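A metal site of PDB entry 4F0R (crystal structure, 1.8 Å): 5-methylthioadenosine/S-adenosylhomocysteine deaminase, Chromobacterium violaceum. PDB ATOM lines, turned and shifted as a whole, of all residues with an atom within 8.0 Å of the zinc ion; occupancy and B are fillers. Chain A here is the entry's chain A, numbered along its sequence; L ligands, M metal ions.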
ATOM      1  N   HIS A  70     -14.482   1.717  -2.632  1.00  0.00           N
ATOM      2  CA  HIS A  70     -13.184   1.266  -2.060  1.00  0.00           C
ATOM      3  C   HIS A  70     -12.962  -0.194  -2.158  1.00  0.00           C
ATOM      4  O   HIS A  70     -13.584  -0.970  -1.401  1.00  0.00           O
ATOM      5  CB  HIS A  70     -13.059   1.719  -0.583  1.00  0.00           C
ATOM      6  CG  HIS A  70     -11.713   1.404   0.035  1.00  0.00           C
ATOM      7  ND1 HIS A  70     -10.591   2.035  -0.345  1.00  0.00           N
ATOM      8  CD2 HIS A  70     -11.313   0.414   0.932  1.00  0.00           C
ATOM      9  CE1 HIS A  70      -9.543   1.529   0.325  1.00  0.00           C
ATOM     10  NE2 HIS A  70      -9.974   0.538   1.076  1.00  0.00           N
ATOM     11  N   GLY A  71     -12.102  -0.579  -3.103  1.00  0.00           N
ATOM     12  CA  GLY A  71     -11.718  -1.991  -3.235  1.00  0.00           C
ATOM     13  C   GLY A  71     -10.239  -2.212  -3.448  1.00  0.00           C
ATOM     14  O   GLY A  71      -9.485  -1.251  -3.688  1.00  0.00           O
ATOM     15  N   HIS A  72      -9.814  -3.466  -3.235  1.00  0.00           N
ATOM     16  CA  HIS A  72      -8.494  -3.974  -3.608  1.00  0.00           C
ATOM     17  C   HIS A  72      -8.718  -5.249  -4.399  1.00  0.00           C
ATOM     18  O   HIS A  72      -8.616  -6.383  -3.868  1.00  0.00           O
ATOM     19  CB  HIS A  72      -7.646  -4.261  -2.372  1.00  0.00           C
ATOM     20  CG  HIS A  72      -7.597  -3.125  -1.390  1.00  0.00           C
ATOM     21  ND1 HIS A  72      -6.973  -1.957  -1.663  1.00  0.00           N
ATOM     22  CD2 HIS A  72      -8.156  -2.991  -0.107  1.00  0.00           C
ATOM     23  CE1 HIS A  72      -7.097  -1.127  -0.601  1.00  0.00           C
ATOM     24  NE2 HIS A  72      -7.891  -1.729   0.319  1.00  0.00           N
ATOM     25  N   MET A  75      -7.076  -8.733  -4.414  1.00  0.00           N
ATOM     26  CA  MET A  75      -7.092  -9.539  -3.203  1.00  0.00           C
ATOM     27  C   MET A  75      -8.225 -10.537  -3.182  1.00  0.00           C
ATOM     28  O   MET A  75      -8.342 -11.337  -2.229  1.00  0.00           O
ATOM     29  CB  MET A  75      -7.119  -8.617  -1.978  1.00  0.00           C
ATOM     30  CG  MET A  75      -5.805  -7.834  -1.975  1.00  0.00           C
ATOM     31  SD  MET A  75      -5.716  -6.738  -0.308  1.00  0.00           S
ATOM     32  CE  MET A  75      -5.095  -8.288   0.810  1.00  0.00           C
ATOM     33  N   MET A 130      -7.662   0.220  -5.440  1.00  0.00           N
ATOM     34  CA  MET A 130      -6.289   0.647  -5.221  1.00  0.00           C
ATOM     35  C   MET A 130      -5.453  -0.541  -4.893  1.00  0.00           C
ATOM     36  O   MET A 130      -5.748  -1.299  -3.993  1.00  0.00           O
ATOM     37  CB  MET A 130      -6.117   1.792  -4.211  1.00  0.00           C
ATOM     38  CG  MET A 130      -6.664   1.440  -2.848  1.00  0.00           C
ATOM     39  SD  MET A 130      -6.492   2.927  -1.555  1.00  0.00           S
ATOM     40  CE  MET A 130      -4.520   2.872  -1.326  1.00  0.00           C
ATOM     41  N   HIS A 192      -1.095   4.995   0.515  1.00  0.00           N
ATOM     42  CA  HIS A 192      -1.804   3.966   1.224  1.00  0.00           C
ATOM     43  C   HIS A 192      -2.496   4.423   2.506  1.00  0.00           C
ATOM     44  O   HIS A 192      -3.698   4.175   2.693  1.00  0.00           O
ATOM     45  CB  HIS A 192      -0.855   2.814   1.513  1.00  0.00           C
ATOM     46  CG  HIS A 192      -1.453   1.782   2.390  1.00  0.00           C
ATOM     47  ND1 HIS A 192      -1.067   1.606   3.681  1.00  0.00           N
ATOM     48  CD2 HIS A 192      -2.478   0.895   2.172  1.00  0.00           C
ATOM     49  CE1 HIS A 192      -1.816   0.667   4.251  1.00  0.00           C
ATOM     50  NE2 HIS A 192      -2.672   0.209   3.333  1.00  0.00           N
ATOM     51  N   HIS A 217      -6.786   8.954  -3.202  1.00  0.00           N
ATOM     52  CA  HIS A 217      -7.554   7.894  -2.594  1.00  0.00           C
ATOM     53  C   HIS A 217      -6.665   7.328  -1.495  1.00  0.00           C
ATOM     54  O   HIS A 217      -5.573   6.816  -1.799  1.00  0.00           O
ATOM     55  CB  HIS A 217      -7.812   6.833  -3.675  1.00  0.00           C
ATOM     56  CG  HIS A 217      -8.630   5.636  -3.215  1.00  0.00           C
ATOM     57  ND1 HIS A 217      -8.819   4.544  -4.003  1.00  0.00           N
ATOM     58  CD2 HIS A 217      -9.293   5.377  -2.014  1.00  0.00           C
ATOM     59  CE1 HIS A 217      -9.558   3.624  -3.328  1.00  0.00           C
ATOM     60  NE2 HIS A 217      -9.840   4.128  -2.117  1.00  0.00           N
ATOM     61  N   CYS A 218      -7.090   7.444  -0.248  1.00  0.00           N
ATOM     62  CA  CYS A 218      -6.179   7.156   0.910  1.00  0.00           C
ATOM     63  C   CYS A 218      -6.962   6.567   2.077  1.00  0.00           C
ATOM     64  O   CYS A 218      -8.083   7.010   2.347  1.00  0.00           O
ATOM     65  CB  CYS A 218      -5.499   8.472   1.336  1.00  0.00           C
ATOM     66  SG  CYS A 218      -4.265   8.294   2.632  1.00  0.00           S
ATOM     67  N   HIS A 219      -6.413   5.554   2.765  1.00  0.00           N
ATOM     68  CA  HIS A 219      -7.061   5.050   3.994  1.00  0.00           C
ATOM     69  C   HIS A 219      -6.793   6.030   5.123  1.00  0.00           C
ATOM     70  O   HIS A 219      -5.633   6.233   5.485  1.00  0.00           O
ATOM     71  CB  HIS A 219      -6.440   3.734   4.430  1.00  0.00           C
ATOM     72  CG  HIS A 219      -6.609   2.597   3.432  1.00  0.00           C
ATOM     73  ND1 HIS A 219      -5.568   2.141   2.678  1.00  0.00           N
ATOM     74  CD2 HIS A 219      -7.684   1.750   3.177  1.00  0.00           C
ATOM     75  CE1 HIS A 219      -5.991   1.086   1.934  1.00  0.00           C
ATOM     76  NE2 HIS A 219      -7.271   0.825   2.247  1.00  0.00           N
ATOM     77  N   GLU A 222      -8.682   4.762  10.107  1.00  0.00           N
ATOM     78  CA  GLU A 222      -9.333   3.438  10.219  1.00  0.00           C
ATOM     79  C   GLU A 222      -9.333   2.888  11.669  1.00  0.00           C
ATOM     80  O   GLU A 222     -10.321   2.286  12.121  1.00  0.00           O
ATOM     81  CB  GLU A 222      -8.671   2.412   9.255  1.00  0.00           C
ATOM     82  CG  GLU A 222      -9.352   1.045   9.317  1.00  0.00           C
ATOM     83  CD  GLU A 222      -8.592  -0.040   8.550  1.00  0.00           C
ATOM     84  OE1 GLU A 222      -7.514   0.241   8.017  1.00  0.00           O
ATOM     85  OE2 GLU A 222      -9.072  -1.186   8.510  1.00  0.00           O
ATOM     86  N   ALA A 255     -10.877   6.749   2.599  1.00  0.00           N
ATOM     87  CA  ALA A 255     -11.458   5.472   2.997  1.00  0.00           C
ATOM     88  C   ALA A 255     -11.459   5.223   4.499  1.00  0.00           C
ATOM     89  O   ALA A 255     -10.533   5.599   5.223  1.00  0.00           O
ATOM     90  CB  ALA A 255     -10.805   4.315   2.212  1.00  0.00           C
ATOM     91  N   HIS A 256     -12.505   4.536   4.943  1.00  0.00           N
ATOM     92  CA  HIS A 256     -12.728   4.177   6.363  1.00  0.00           C
ATOM     93  C   HIS A 256     -13.272   5.306   7.220  1.00  0.00           C
ATOM     94  O   HIS A 256     -14.446   5.319   7.535  1.00  0.00           O
ATOM     95  CB  HIS A 256     -11.500   3.508   7.015  1.00  0.00           C
ATOM     96  CG  HIS A 256     -11.131   2.213   6.374  1.00  0.00           C
ATOM     97  ND1 HIS A 256     -11.990   1.203   6.245  1.00  0.00           N
ATOM     98  CD2 HIS A 256      -9.935   1.782   5.765  1.00  0.00           C
ATOM     99  CE1 HIS A 256     -11.384   0.155   5.629  1.00  0.00           C
ATOM    100  NE2 HIS A 256     -10.145   0.525   5.302  1.00  0.00           N
ATOM    101  N   ASN A 278     -16.825   1.356   4.873  1.00  0.00           N
ATOM    102  CA  ASN A 278     -16.566  -0.034   4.565  1.00  0.00           C
ATOM    103  C   ASN A 278     -16.981  -0.905   5.744  1.00  0.00           C
ATOM    104  O   ASN A 278     -16.122  -1.350   6.516  1.00  0.00           O
ATOM    105  CB  ASN A 278     -15.072  -0.239   4.244  1.00  0.00           C
ATOM    106  CG  ASN A 278     -14.574   0.722   3.157  1.00  0.00           C
ATOM    107  OD1 ASN A 278     -15.104   0.756   2.057  1.00  0.00           O
ATOM    108  ND2 ASN A 278     -13.582   1.501   3.487  1.00  0.00           N
ATOM    109  N   SER A 281     -15.636  -4.743   6.556  1.00  0.00           N
ATOM    110  CA  SER A 281     -14.197  -4.750   6.866  1.00  0.00           C
ATOM    111  C   SER A 281     -13.963  -4.115   8.248  1.00  0.00           C
ATOM    112  O   SER A 281     -13.175  -4.599   9.040  1.00  0.00           O
ATOM    113  CB  SER A 281     -13.434  -3.983   5.789  1.00  0.00           C
ATOM    114  OG  SER A 281     -12.049  -4.040   6.078  1.00  0.00           O
ATOM    115  N   LEU A 285     -12.452  -6.585  10.972  1.00  0.00           N
ATOM    116  CA  LEU A 285     -11.139  -6.212  11.544  1.00  0.00           C
ATOM    117  C   LEU A 285     -11.262  -5.497  12.911  1.00  0.00           C
ATOM    118  O   LEU A 285     -10.245  -5.156  13.502  1.00  0.00           O
ATOM    119  CB  LEU A 285     -10.302  -5.379  10.534  1.00  0.00           C
ATOM    120  CG  LEU A 285     -10.085  -6.053   9.149  1.00  0.00           C
ATOM    121  CD1 LEU A 285      -9.240  -5.202   8.193  1.00  0.00           C
ATOM    122  CD2 LEU A 285      -9.504  -7.449   9.284  1.00  0.00           C
ATOM    123  N   THR A 306     -16.446  -2.093  -0.327  1.00  0.00           N
ATOM    124  CA  THR A 306     -16.410  -3.411   0.281  1.00  0.00           C
ATOM    125  C   THR A 306     -15.052  -3.673   0.939  1.00  0.00           C
ATOM    126  O   THR A 306     -14.942  -4.621   1.695  1.00  0.00           O
ATOM    127  CB  THR A 306     -16.614  -4.500  -0.772  1.00  0.00           C
ATOM    128  OG1 THR A 306     -15.628  -4.357  -1.812  1.00  0.00           O
ATOM    129  CG2 THR A 306     -18.044  -4.380  -1.397  1.00  0.00           C
ATOM    130  N   ASP A 307     -14.049  -2.865   0.594  1.00  0.00           N
ATOM    131  CA  ASP A 307     -12.633  -3.153   0.864  1.00  0.00           C
ATOM    132  C   ASP A 307     -12.262  -4.438   0.113  1.00  0.00           C
ATOM    133  O   ASP A 307     -12.976  -4.867  -0.812  1.00  0.00           O
ATOM    134  CB  ASP A 307     -12.388  -3.313   2.384  1.00  0.00           C
ATOM    135  CG  ASP A 307     -11.029  -2.751   2.849  1.00  0.00           C
ATOM    136  OD1 ASP A 307     -10.222  -2.200   2.043  1.00  0.00           O
ATOM    137  OD2 ASP A 307     -10.815  -2.841   4.075  1.00  0.00           O
ATOM    138  N   GLY A 308     -11.170  -5.056   0.523  1.00  0.00           N
ATOM    139  CA  GLY A 308     -10.681  -6.297  -0.153  1.00  0.00           C
ATOM    140  C   GLY A 308     -11.441  -7.561   0.289  1.00  0.00           C
ATOM    141  O   GLY A 308     -11.952  -7.640   1.426  1.00  0.00           O
ATOM    142  N   SER A 311     -11.067  -9.342   3.751  1.00  0.00           N
ATOM    143  CA  SER A 311     -11.667  -8.895   4.995  1.00  0.00           C
ATOM    144  C   SER A 311     -13.087  -8.415   4.768  1.00  0.00           C
ATOM    145  O   SER A 311     -13.415  -7.259   4.960  1.00  0.00           O
ATOM    146  CB  SER A 311     -10.805  -7.828   5.673  1.00  0.00           C
ATOM    147  OG  SER A 311     -10.784  -6.648   4.913  1.00  0.00           O
HETATM  148  C1  LIG L   1      -2.898  -0.829  -1.543  1.00  0.00           C
HETATM  149  S1  LIG L   1      -3.635  -1.797  -0.287  1.00  0.00           S
HETATM  150  C2  LIG L   1      -2.318  -2.179   0.846  1.00  0.00           C
HETATM  151  C3  LIG L   1      -1.382  -3.191   0.224  1.00  0.00           C
HETATM  152  O1  LIG L   1      -0.048  -3.076   0.824  1.00  0.00           O
HETATM  153  C4  LIG L   1      -1.264  -4.752   1.942  1.00  0.00           C
HETATM  154  O2  LIG L   1      -1.230  -6.113   2.319  1.00  0.00           O
HETATM  155  C5  LIG L   1      -1.888  -4.569   0.578  1.00  0.00           C
HETATM  156  O3  LIG L   1      -1.314  -5.525  -0.328  1.00  0.00           O
HETATM  157  C6  LIG L   1       0.120  -4.150   1.755  1.00  0.00           C
HETATM  158  N1  LIG L   1       0.650  -3.633   3.031  1.00  0.00           N
HETATM  159  C7  LIG L   1       0.132  -2.614   3.769  1.00  0.00           C
HETATM  160  N2  LIG L   1       0.920  -2.375   4.879  1.00  0.00           N
HETATM  161  C8  LIG L   1       1.934  -3.259   4.842  1.00  0.00           C
HETATM  162  C9  LIG L   1       3.122  -3.573   5.695  1.00  0.00           C
HETATM  163  N3  LIG L   1       3.374  -2.885   6.823  1.00  0.00           N
HETATM  164  N4  LIG L   1       3.945  -4.580   5.291  1.00  0.00           N
HETATM  165  C10 LIG L   1       3.726  -5.293   4.160  1.00  0.00           C
HETATM  166  N5  LIG L   1       2.698  -5.040   3.325  1.00  0.00           N
HETATM  167  C11 LIG L   1       1.784  -4.061   3.618  1.00  0.00           C
HETATM  168 ZN    ZN M   1      -8.691  -0.775   1.904  1.00  0.00          ZN
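A ring nitrogen (ND1) of His 72 lies close to a sulfur (S1) of the ligand (3.6 Å).
The backbone carbonyl oxygen (O) of His 70 lies within hydrogen-bond range of the backbone NH (N) of Thr 306. A ring nitrogen (ND1) of His 70 lies within hydrogen-bond range of a ring nitrogen (NE2) of His 217, at 2.8 Å. ND1 of His 219 lies within hydrogen-bond range of O of His 192. The side-chain hydroxyl of Ser 281 is in hydrogen-bond range of the side-chain carboxylate of Asp 307 (2.6 Å). ND2 of Asn 278 lies within hydrogen-bond range of ND1 of His 256, at 3.2 Å. O of Met 130 lies within hydrogen-bond range of ND1 of His 72, 2.7 Å away.
His 256 touches the zinc ion. Of the 19 residues printed, 5 come within 4 Å of the zinc ion.
The zinc ion is bound by a ring nitrogen (NE2) of His 70 (2.0 Å), a ring nitrogen (NE2) of His 72 (2.0 Å), the side-chain carboxylate of Asp 307 (2.1 Å) and a ring nitrogen (NE2) of His 219 (2.2 Å). The zinc ion has four donor atoms within binding distance.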
